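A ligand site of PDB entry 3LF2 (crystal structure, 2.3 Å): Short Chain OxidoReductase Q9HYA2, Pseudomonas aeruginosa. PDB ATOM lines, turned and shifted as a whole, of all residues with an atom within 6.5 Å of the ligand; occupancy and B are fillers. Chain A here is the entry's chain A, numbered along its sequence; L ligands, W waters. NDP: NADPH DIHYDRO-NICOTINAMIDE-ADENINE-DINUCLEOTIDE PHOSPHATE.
The backbone NH (N) of Asp 41 is in hydrogen-bond range of an oxygen (O3X) of the ligand.
N of Ser 17 is in hydrogen-bond range of O3B of the ligand.
O3B of the ligand is in hydrogen-bond range of OG of Ser 17 (2.8 Å).
The backbone NH of Arg 40 sits at hydrogen-bond distance from an oxygen (O2X) of the ligand.
The guanidinium group (NE) of Arg 40 lies within salt-bridge range of an oxygen (O2X) of the ligand (2.8 Å).
A nitrogen (N6A) of the ligand sits at hydrogen-bond distance from the side-chain carboxylate (OD1) of Asp 67 (3.0 Å).
N of Val 68 is in hydrogen-bond range of N1A of the ligand.
The guanidinium group (NH2) of Arg 44 lies within salt-bridge range of an oxygen (O1X) of the ligand (3.2 Å).
N of Ser 18 lies within hydrogen-bond range of O3B of the ligand (3.4 Å).
The backbone NH (N) of Arg 44 is in hydrogen-bond range of the side-chain carboxylate (OD2) of Asp 41.
OG of Ser 17 sits at hydrogen-bond distance from NE of Arg 44 (3.4 Å).
N of Leu 69 is in hydrogen-bond range of OD1 of Asp 67 (2.8 Å).
O of Ala 39 sits at hydrogen-bond distance from N of Cys 66 (2.9 Å).
The backbone carbonyl oxygen of Gly 15 lies close to the side-chain amide oxygen of Asn 94 (2.7 Å).
The backbone carbonyl oxygen (O) of Cys 38 lies within hydrogen-bond range of the backbone NH (N) of Gly 15.
The backbone carbonyl oxygen (O) of Thr 14 is in hydrogen-bond range of the backbone NH (N) of Ala 95 (3.2 Å).
Gly 15 touches the ligand (CA to O4B, 3.2 Å).
Ala 39 touches the ligand (CB to O2B, 3.3 Å).
Cys 66 touches the ligand (O to C2A, 3.2 Å).
CB of Ala 95 touches C4A of the ligand (3.7 Å).
Gly 96 touches the ligand (O to O2A, 3.5 Å).
Gln 97 touches the ligand.
Hydrophobic or aromatic side chains that line the ligand: Ala 39, Val 68 and Ala 95.
Of the 29 residues printed, 13 come within 4 Å of the ligand.
The nearest printed residue that does not touch the ligand is Asn 94 (4.01 Å).
Water W1 lies within hydrogen-bond range of OD1 of Asn 94 (2.6 Å), O of Ser 18 (3.0 Å), N of Gly 21 (3.0 Å) and N of Ile 20 (3.5 Å).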
ATOM      1  N   THR A  14      12.951 -18.402 -23.660  1.00  0.00           N
ATOM      2  CA  THR A  14      12.050 -19.106 -24.561  1.00  0.00           C
ATOM      3  C   THR A  14      11.250 -20.144 -23.791  1.00  0.00           C
ATOM      4  O   THR A  14      11.788 -20.867 -22.977  1.00  0.00           O
ATOM      5  CB  THR A  14      12.823 -19.791 -25.675  1.00  0.00           C
ATOM      6  OG1 THR A  14      13.534 -20.918 -25.142  1.00  0.00           O
ATOM      7  CG2 THR A  14      13.816 -18.823 -26.284  1.00  0.00           C
ATOM      8  N   GLY A  15       9.949 -20.203 -24.038  1.00  0.00           N
ATOM      9  CA  GLY A  15       9.100 -21.105 -23.272  1.00  0.00           C
ATOM     10  C   GLY A  15       8.850 -20.544 -21.889  1.00  0.00           C
ATOM     11  O   GLY A  15       8.878 -21.269 -20.901  1.00  0.00           O
ATOM     12  N   GLY A  16       8.576 -19.241 -21.822  1.00  0.00           N
ATOM     13  CA  GLY A  16       8.463 -18.558 -20.541  1.00  0.00           C
ATOM     14  C   GLY A  16       7.072 -18.356 -19.965  1.00  0.00           C
ATOM     15  O   GLY A  16       6.907 -17.676 -18.951  1.00  0.00           O
ATOM     16  N   SER A  17       6.051 -18.949 -20.584  1.00  0.00           N
ATOM     17  CA  SER A  17       4.673 -18.702 -20.147  1.00  0.00           C
ATOM     18  C   SER A  17       4.144 -19.619 -19.036  1.00  0.00           C
ATOM     19  O   SER A  17       3.039 -19.406 -18.530  1.00  0.00           O
ATOM     20  CB  SER A  17       3.700 -18.693 -21.342  1.00  0.00           C
ATOM     21  OG  SER A  17       3.387 -20.013 -21.740  1.00  0.00           O
ATOM     22  N   SER A  18       4.919 -20.642 -18.669  1.00  0.00           N
ATOM     23  CA  SER A  18       4.550 -21.523 -17.556  1.00  0.00           C
ATOM     24  C   SER A  18       5.709 -22.394 -17.088  1.00  0.00           C
ATOM     25  O   SER A  18       6.779 -22.385 -17.668  1.00  0.00           O
ATOM     26  CB  SER A  18       3.374 -22.431 -17.938  1.00  0.00           C
ATOM     27  OG  SER A  18       3.808 -23.506 -18.749  1.00  0.00           O
ATOM     28  N   GLY A  19       5.460 -23.149 -16.016  1.00  0.00           N
ATOM     29  CA  GLY A  19       6.441 -24.055 -15.448  1.00  0.00           C
ATOM     30  C   GLY A  19       7.787 -23.417 -15.139  1.00  0.00           C
ATOM     31  O   GLY A  19       7.860 -22.289 -14.637  1.00  0.00           O
ATOM     32  N   ILE A  20       8.842 -24.151 -15.439  1.00  0.00           N
ATOM     33  CA  ILE A  20      10.217 -23.706 -15.198  1.00  0.00           C
ATOM     34  C   ILE A  20      10.510 -22.383 -15.910  1.00  0.00           C
ATOM     35  O   ILE A  20      11.240 -21.541 -15.396  1.00  0.00           O
ATOM     36  CB  ILE A  20      11.225 -24.814 -15.629  1.00  0.00           C
ATOM     37  CG1 ILE A  20      11.025 -26.076 -14.797  1.00  0.00           C
ATOM     38  CG2 ILE A  20      12.672 -24.352 -15.493  1.00  0.00           C
ATOM     39  CD1 ILE A  20      11.920 -27.260 -15.204  1.00  0.00           C
ATOM     40  N   GLY A  21       9.970 -22.196 -17.114  1.00  0.00           N
ATOM     41  CA  GLY A  21      10.195 -20.962 -17.835  1.00  0.00           C
ATOM     42  C   GLY A  21       9.614 -19.730 -17.126  1.00  0.00           C
ATOM     43  O   GLY A  21      10.290 -18.707 -16.969  1.00  0.00           O
ATOM     44  N   LEU A  22       8.356 -19.850 -16.693  1.00  0.00           N
ATOM     45  CA  LEU A  22       7.693 -18.786 -15.936  1.00  0.00           C
ATOM     46  C   LEU A  22       8.397 -18.525 -14.602  1.00  0.00           C
ATOM     47  O   LEU A  22       8.630 -17.372 -14.215  1.00  0.00           O
ATOM     48  CB  LEU A  22       6.220 -19.134 -15.691  1.00  0.00           C
ATOM     49  CG  LEU A  22       5.388 -18.073 -14.974  1.00  0.00           C
ATOM     50  CD1 LEU A  22       5.553 -16.723 -15.655  1.00  0.00           C
ATOM     51  CD2 LEU A  22       3.917 -18.489 -14.927  1.00  0.00           C
ATOM     52  N   CYS A  38       8.787 -15.753 -24.691  1.00  0.00           N
ATOM     53  CA  CYS A  38       7.935 -16.153 -25.789  1.00  0.00           C
ATOM     54  C   CYS A  38       7.318 -17.509 -25.521  1.00  0.00           C
ATOM     55  O   CYS A  38       7.740 -18.248 -24.644  1.00  0.00           O
ATOM     56  CB  CYS A  38       8.697 -16.155 -27.121  1.00  0.00           C
ATOM     57  SG  CYS A  38       9.915 -17.512 -27.355  1.00  0.00           S
ATOM     58  N   ALA A  39       6.295 -17.826 -26.298  1.00  0.00           N
ATOM     59  CA  ALA A  39       5.629 -19.120 -26.262  1.00  0.00           C
ATOM     60  C   ALA A  39       4.617 -19.086 -27.382  1.00  0.00           C
ATOM     61  O   ALA A  39       4.358 -18.017 -27.969  1.00  0.00           O
ATOM     62  CB  ALA A  39       4.954 -19.334 -24.918  1.00  0.00           C
ATOM     63  N   ARG A  40       4.014 -20.225 -27.666  1.00  0.00           N
ATOM     64  CA  ARG A  40       3.121 -20.326 -28.805  1.00  0.00           C
ATOM     65  C   ARG A  40       1.716 -19.835 -28.470  1.00  0.00           C
ATOM     66  O   ARG A  40       1.126 -19.096 -29.258  1.00  0.00           O
ATOM     67  CB  ARG A  40       3.105 -21.761 -29.356  1.00  0.00           C
ATOM     68  CG  ARG A  40       4.468 -22.216 -29.880  1.00  0.00           C
ATOM     69  CD  ARG A  40       4.517 -23.707 -30.128  1.00  0.00           C
ATOM     70  NE  ARG A  40       4.298 -24.477 -28.904  1.00  0.00           N
ATOM     71  CZ  ARG A  40       3.983 -25.768 -28.875  1.00  0.00           C
ATOM     72  NH1 ARG A  40       3.821 -26.432 -30.013  1.00  0.00           N
ATOM     73  NH2 ARG A  40       3.792 -26.381 -27.708  1.00  0.00           N
ATOM     74  N   ASP A  41       1.206 -20.217 -27.301  1.00  0.00           N
ATOM     75  CA  ASP A  41      -0.156 -19.876 -26.904  1.00  0.00           C
ATOM     76  C   ASP A  41      -0.278 -18.423 -26.428  1.00  0.00           C
ATOM     77  O   ASP A  41       0.067 -18.102 -25.300  1.00  0.00           O
ATOM     78  CB  ASP A  41      -0.649 -20.834 -25.827  1.00  0.00           C
ATOM     79  CG  ASP A  41      -2.079 -20.555 -25.387  1.00  0.00           C
ATOM     80  OD1 ASP A  41      -2.668 -21.428 -24.731  1.00  0.00           O
ATOM     81  OD2 ASP A  41      -2.622 -19.462 -25.693  1.00  0.00           O
ATOM     82  N   GLY A  42      -0.788 -17.572 -27.310  1.00  0.00           N
ATOM     83  CA  GLY A  42      -0.902 -16.143 -27.037  1.00  0.00           C
ATOM     84  C   GLY A  42      -1.663 -15.766 -25.787  1.00  0.00           C
ATOM     85  O   GLY A  42      -1.306 -14.798 -25.113  1.00  0.00           O
ATOM     86  N   ARG A  44      -2.356 -17.694 -22.889  1.00  0.00           N
ATOM     87  CA  ARG A  44      -1.623 -18.071 -21.680  1.00  0.00           C
ATOM     88  C   ARG A  44      -0.443 -17.111 -21.527  1.00  0.00           C
ATOM     89  O   ARG A  44      -0.089 -16.710 -20.423  1.00  0.00           O
ATOM     90  CB  ARG A  44      -1.155 -19.535 -21.748  1.00  0.00           C
ATOM     91  CG  ARG A  44      -0.723 -20.086 -20.398  1.00  0.00           C
ATOM     92  CD  ARG A  44      -0.545 -21.598 -20.419  1.00  0.00           C
ATOM     93  NE  ARG A  44       0.657 -22.015 -21.134  1.00  0.00           N
ATOM     94  CZ  ARG A  44       1.063 -23.278 -21.257  1.00  0.00           C
ATOM     95  NH1 ARG A  44       0.358 -24.258 -20.700  1.00  0.00           N
ATOM     96  NH2 ARG A  44       2.171 -23.553 -21.931  1.00  0.00           N
ATOM     97  N   LEU A  45       0.144 -16.742 -22.660  1.00  0.00           N
ATOM     98  CA  LEU A  45       1.271 -15.816 -22.726  1.00  0.00           C
ATOM     99  C   LEU A  45       0.908 -14.450 -22.136  1.00  0.00           C
ATOM    100  O   LEU A  45       1.636 -13.918 -21.300  1.00  0.00           O
ATOM    101  CB  LEU A  45       1.693 -15.671 -24.180  1.00  0.00           C
ATOM    102  CG  LEU A  45       2.886 -14.841 -24.672  1.00  0.00           C
ATOM    103  CD1 LEU A  45       2.650 -13.351 -24.532  1.00  0.00           C
ATOM    104  CD2 LEU A  45       4.167 -15.268 -23.993  1.00  0.00           C
ATOM    105  N   CYS A  66       5.769 -16.733 -30.183  1.00  0.00           N
ATOM    106  CA  CYS A  66       6.859 -17.204 -31.038  1.00  0.00           C
ATOM    107  C   CYS A  66       7.041 -18.702 -30.871  1.00  0.00           C
ATOM    108  O   CYS A  66       7.118 -19.201 -29.750  1.00  0.00           O
ATOM    109  CB  CYS A  66       8.174 -16.467 -30.706  1.00  0.00           C
ATOM    110  SG  CYS A  66       9.609 -16.941 -31.750  1.00  0.00           S
ATOM    111  N   ASP A  67       7.085 -19.420 -31.998  1.00  0.00           N
ATOM    112  CA  ASP A  67       7.396 -20.836 -31.970  1.00  0.00           C
ATOM    113  C   ASP A  67       8.888 -20.998 -32.314  1.00  0.00           C
ATOM    114  O   ASP A  67       9.297 -20.726 -33.439  1.00  0.00           O
ATOM    115  CB  ASP A  67       6.494 -21.611 -32.953  1.00  0.00           C
ATOM    116  CG  ASP A  67       6.874 -23.104 -33.075  1.00  0.00           C
ATOM    117  OD1 ASP A  67       7.873 -23.555 -32.477  1.00  0.00           O
ATOM    118  OD2 ASP A  67       6.144 -23.827 -33.791  1.00  0.00           O
ATOM    119  N   VAL A  68       9.679 -21.437 -31.340  1.00  0.00           N
ATOM    120  CA  VAL A  68      11.131 -21.524 -31.534  1.00  0.00           C
ATOM    121  C   VAL A  68      11.548 -22.485 -32.660  1.00  0.00           C
ATOM    122  O   VAL A  68      12.665 -22.420 -33.151  1.00  0.00           O
ATOM    123  CB  VAL A  68      11.861 -21.897 -30.220  1.00  0.00           C
ATOM    124  CG1 VAL A  68      11.574 -20.850 -29.144  1.00  0.00           C
ATOM    125  CG2 VAL A  68      11.445 -23.290 -29.744  1.00  0.00           C
ATOM    126  N   LEU A  69      10.622 -23.341 -33.078  1.00  0.00           N
ATOM    127  CA  LEU A  69      10.879 -24.241 -34.202  1.00  0.00           C
ATOM    128  C   LEU A  69      10.932 -23.501 -35.535  1.00  0.00           C
ATOM    129  O   LEU A  69      11.444 -24.036 -36.530  1.00  0.00           O
ATOM    130  CB  LEU A  69       9.834 -25.361 -34.255  1.00  0.00           C
ATOM    131  CG  LEU A  69      10.124 -26.698 -33.564  1.00  0.00           C
ATOM    132  CD1 LEU A  69      10.871 -26.525 -32.245  1.00  0.00           C
ATOM    133  CD2 LEU A  69       8.822 -27.460 -33.343  1.00  0.00           C
ATOM    134  N   ASN A  94      14.367 -22.901 -22.754  1.00  0.00           N
ATOM    135  CA  ASN A  94      13.599 -23.760 -21.864  1.00  0.00           C
ATOM    136  C   ASN A  94      12.615 -24.628 -22.630  1.00  0.00           C
ATOM    137  O   ASN A  94      12.464 -25.818 -22.336  1.00  0.00           O
ATOM    138  CB  ASN A  94      12.885 -22.899 -20.802  1.00  0.00           C
ATOM    139  CG  ASN A  94      11.718 -23.617 -20.167  1.00  0.00           C
ATOM    140  OD1 ASN A  94      10.558 -23.268 -20.404  1.00  0.00           O
ATOM    141  ND2 ASN A  94      12.014 -24.617 -19.347  1.00  0.00           N
ATOM    142  N   ALA A  95      11.954 -24.029 -23.615  1.00  0.00           N
ATOM    143  CA  ALA A  95      11.004 -24.733 -24.484  1.00  0.00           C
ATOM    144  C   ALA A  95      11.438 -26.172 -24.739  1.00  0.00           C
ATOM    145  O   ALA A  95      12.608 -26.445 -25.029  1.00  0.00           O
ATOM    146  CB  ALA A  95      10.820 -23.981 -25.814  1.00  0.00           C
ATOM    147  N   GLY A  96      10.480 -27.095 -24.634  1.00  0.00           N
ATOM    148  CA  GLY A  96      10.756 -28.517 -24.746  1.00  0.00           C
ATOM    149  C   GLY A  96       9.619 -29.318 -24.140  1.00  0.00           C
ATOM    150  O   GLY A  96       8.918 -28.843 -23.257  1.00  0.00           O
ATOM    151  N   GLN A  97       9.432 -30.534 -24.636  1.00  0.00           N
ATOM    152  CA  GLN A  97       8.385 -31.414 -24.131  1.00  0.00           C
ATOM    153  C   GLN A  97       8.782 -32.867 -24.269  1.00  0.00           C
ATOM    154  O   GLN A  97       8.858 -33.403 -25.377  1.00  0.00           O
ATOM    155  CB  GLN A  97       7.050 -31.145 -24.857  1.00  0.00           C
ATOM    156  CG  GLN A  97       7.158 -31.095 -26.374  1.00  0.00           C
ATOM    157  CD  GLN A  97       5.794 -30.909 -27.045  1.00  0.00           C
ATOM    158  OE1 GLN A  97       4.756 -31.110 -26.421  1.00  0.00           O
ATOM    159  NE2 GLN A  97       5.814 -30.518 -28.312  1.00  0.00           N
ATOM    160  N   GLY A  98       9.049 -33.512 -23.138  1.00  0.00           N
ATOM    161  CA  GLY A  98       9.516 -34.890 -23.131  1.00  0.00           C
ATOM    162  C   GLY A  98       8.556 -35.820 -23.828  1.00  0.00           C
ATOM    163  O   GLY A  98       7.416 -35.454 -24.121  1.00  0.00           O
ATOM    164  N   LEU A 117      12.803 -31.028 -32.220  1.00  0.00           N
ATOM    165  CA  LEU A 117      12.337 -30.215 -31.099  1.00  0.00           C
ATOM    166  C   LEU A 117      13.468 -29.977 -30.111  1.00  0.00           C
ATOM    167  O   LEU A 117      13.765 -28.845 -29.736  1.00  0.00           O
ATOM    168  CB  LEU A 117      11.142 -30.894 -30.423  1.00  0.00           C
ATOM    169  CG  LEU A 117      10.383 -30.254 -29.254  1.00  0.00           C
ATOM    170  CD1 LEU A 117      10.991 -30.654 -27.919  1.00  0.00           C
ATOM    171  CD2 LEU A 117      10.324 -28.746 -29.377  1.00  0.00           C
ATOM    172  N   SER A 121      15.004 -25.943 -30.824  1.00  0.00           N
ATOM    173  CA  SER A 121      14.576 -25.058 -29.756  1.00  0.00           C
ATOM    174  C   SER A 121      15.810 -24.420 -29.068  1.00  0.00           C
ATOM    175  O   SER A 121      15.679 -23.426 -28.346  1.00  0.00           O
ATOM    176  CB  SER A 121      13.696 -25.810 -28.764  1.00  0.00           C
ATOM    177  OG  SER A 121      14.407 -26.908 -28.219  1.00  0.00           O
ATOM    178  N   SER A 194       4.722 -30.878 -12.675  1.00  0.00           N
ATOM    179  CA  SER A 194       4.358 -30.263 -13.938  1.00  0.00           C
ATOM    180  C   SER A 194       2.911 -30.553 -14.299  1.00  0.00           C
ATOM    181  O   SER A 194       2.247 -31.334 -13.610  1.00  0.00           O
ATOM    182  CB  SER A 194       5.266 -30.768 -15.074  1.00  0.00           C
ATOM    183  OG  SER A 194       5.036 -32.151 -15.316  1.00  0.00           O
ATOM    184  N   GLY A 195       2.446 -29.941 -15.380  1.00  0.00           N
ATOM    185  CA  GLY A 195       1.106 -30.187 -15.871  1.00  0.00           C
ATOM    186  C   GLY A 195       0.921 -31.666 -16.133  1.00  0.00           C
ATOM    187  O   GLY A 195      -0.109 -32.246 -15.794  1.00  0.00           O
HETATM  188  PA  NDP L   1       5.433 -27.361 -21.805  1.00  0.00           P
HETATM  189  O1A NDP L   1       4.079 -26.807 -21.597  1.00  0.00           O
HETATM  190  O2A NDP L   1       5.447 -28.322 -22.933  1.00  0.00           O
HETATM  191  O5B NDP L   1       6.501 -26.177 -22.066  1.00  0.00           O
HETATM  192  C5B NDP L   1       6.736 -25.157 -21.115  1.00  0.00           C
HETATM  193  C4B NDP L   1       6.845 -23.803 -21.810  1.00  0.00           C
HETATM  194  O4B NDP L   1       7.493 -23.920 -23.060  1.00  0.00           O
HETATM  195  C3B NDP L   1       5.452 -23.257 -22.083  1.00  0.00           C
HETATM  196  O3B NDP L   1       5.439 -21.877 -21.781  1.00  0.00           O
HETATM  197  C2B NDP L   1       5.252 -23.471 -23.569  1.00  0.00           C
HETATM  198  O2B NDP L   1       4.363 -22.516 -24.094  1.00  0.00           O
HETATM  199  C1B NDP L   1       6.687 -23.361 -24.091  1.00  0.00           C
HETATM  200  N9A NDP L   1       6.865 -24.012 -25.408  1.00  0.00           N
HETATM  201  C8A NDP L   1       6.645 -25.337 -25.696  1.00  0.00           C
HETATM  202  N7A NDP L   1       6.915 -25.557 -27.006  1.00  0.00           N
HETATM  203  C5A NDP L   1       7.304 -24.390 -27.565  1.00  0.00           C
HETATM  204  C6A NDP L   1       7.685 -24.058 -28.871  1.00  0.00           C
HETATM  205  N6A NDP L   1       7.717 -24.995 -29.821  1.00  0.00           N
HETATM  206  N1A NDP L   1       8.042 -22.764 -29.169  1.00  0.00           N
HETATM  207  C2A NDP L   1       8.013 -21.808 -28.172  1.00  0.00           C
HETATM  208  N3A NDP L   1       7.631 -22.132 -26.877  1.00  0.00           N
HETATM  209  C4A NDP L   1       7.277 -23.404 -26.574  1.00  0.00           C
HETATM  210  O3  NDP L   1       5.939 -28.071 -20.440  1.00  0.00           O
HETATM  211  P2B NDP L   1       3.360 -22.929 -25.281  1.00  0.00           P
HETATM  212  O1X NDP L   1       2.760 -24.292 -24.975  1.00  0.00           O
HETATM  213  O2X NDP L   1       4.151 -22.965 -26.567  1.00  0.00           O
HETATM  214  O3X NDP L   1       2.246 -21.913 -25.440  1.00  0.00           O
HETATM  215  O   HOH W   1       8.725 -24.296 -18.896  1.00  0.00           O
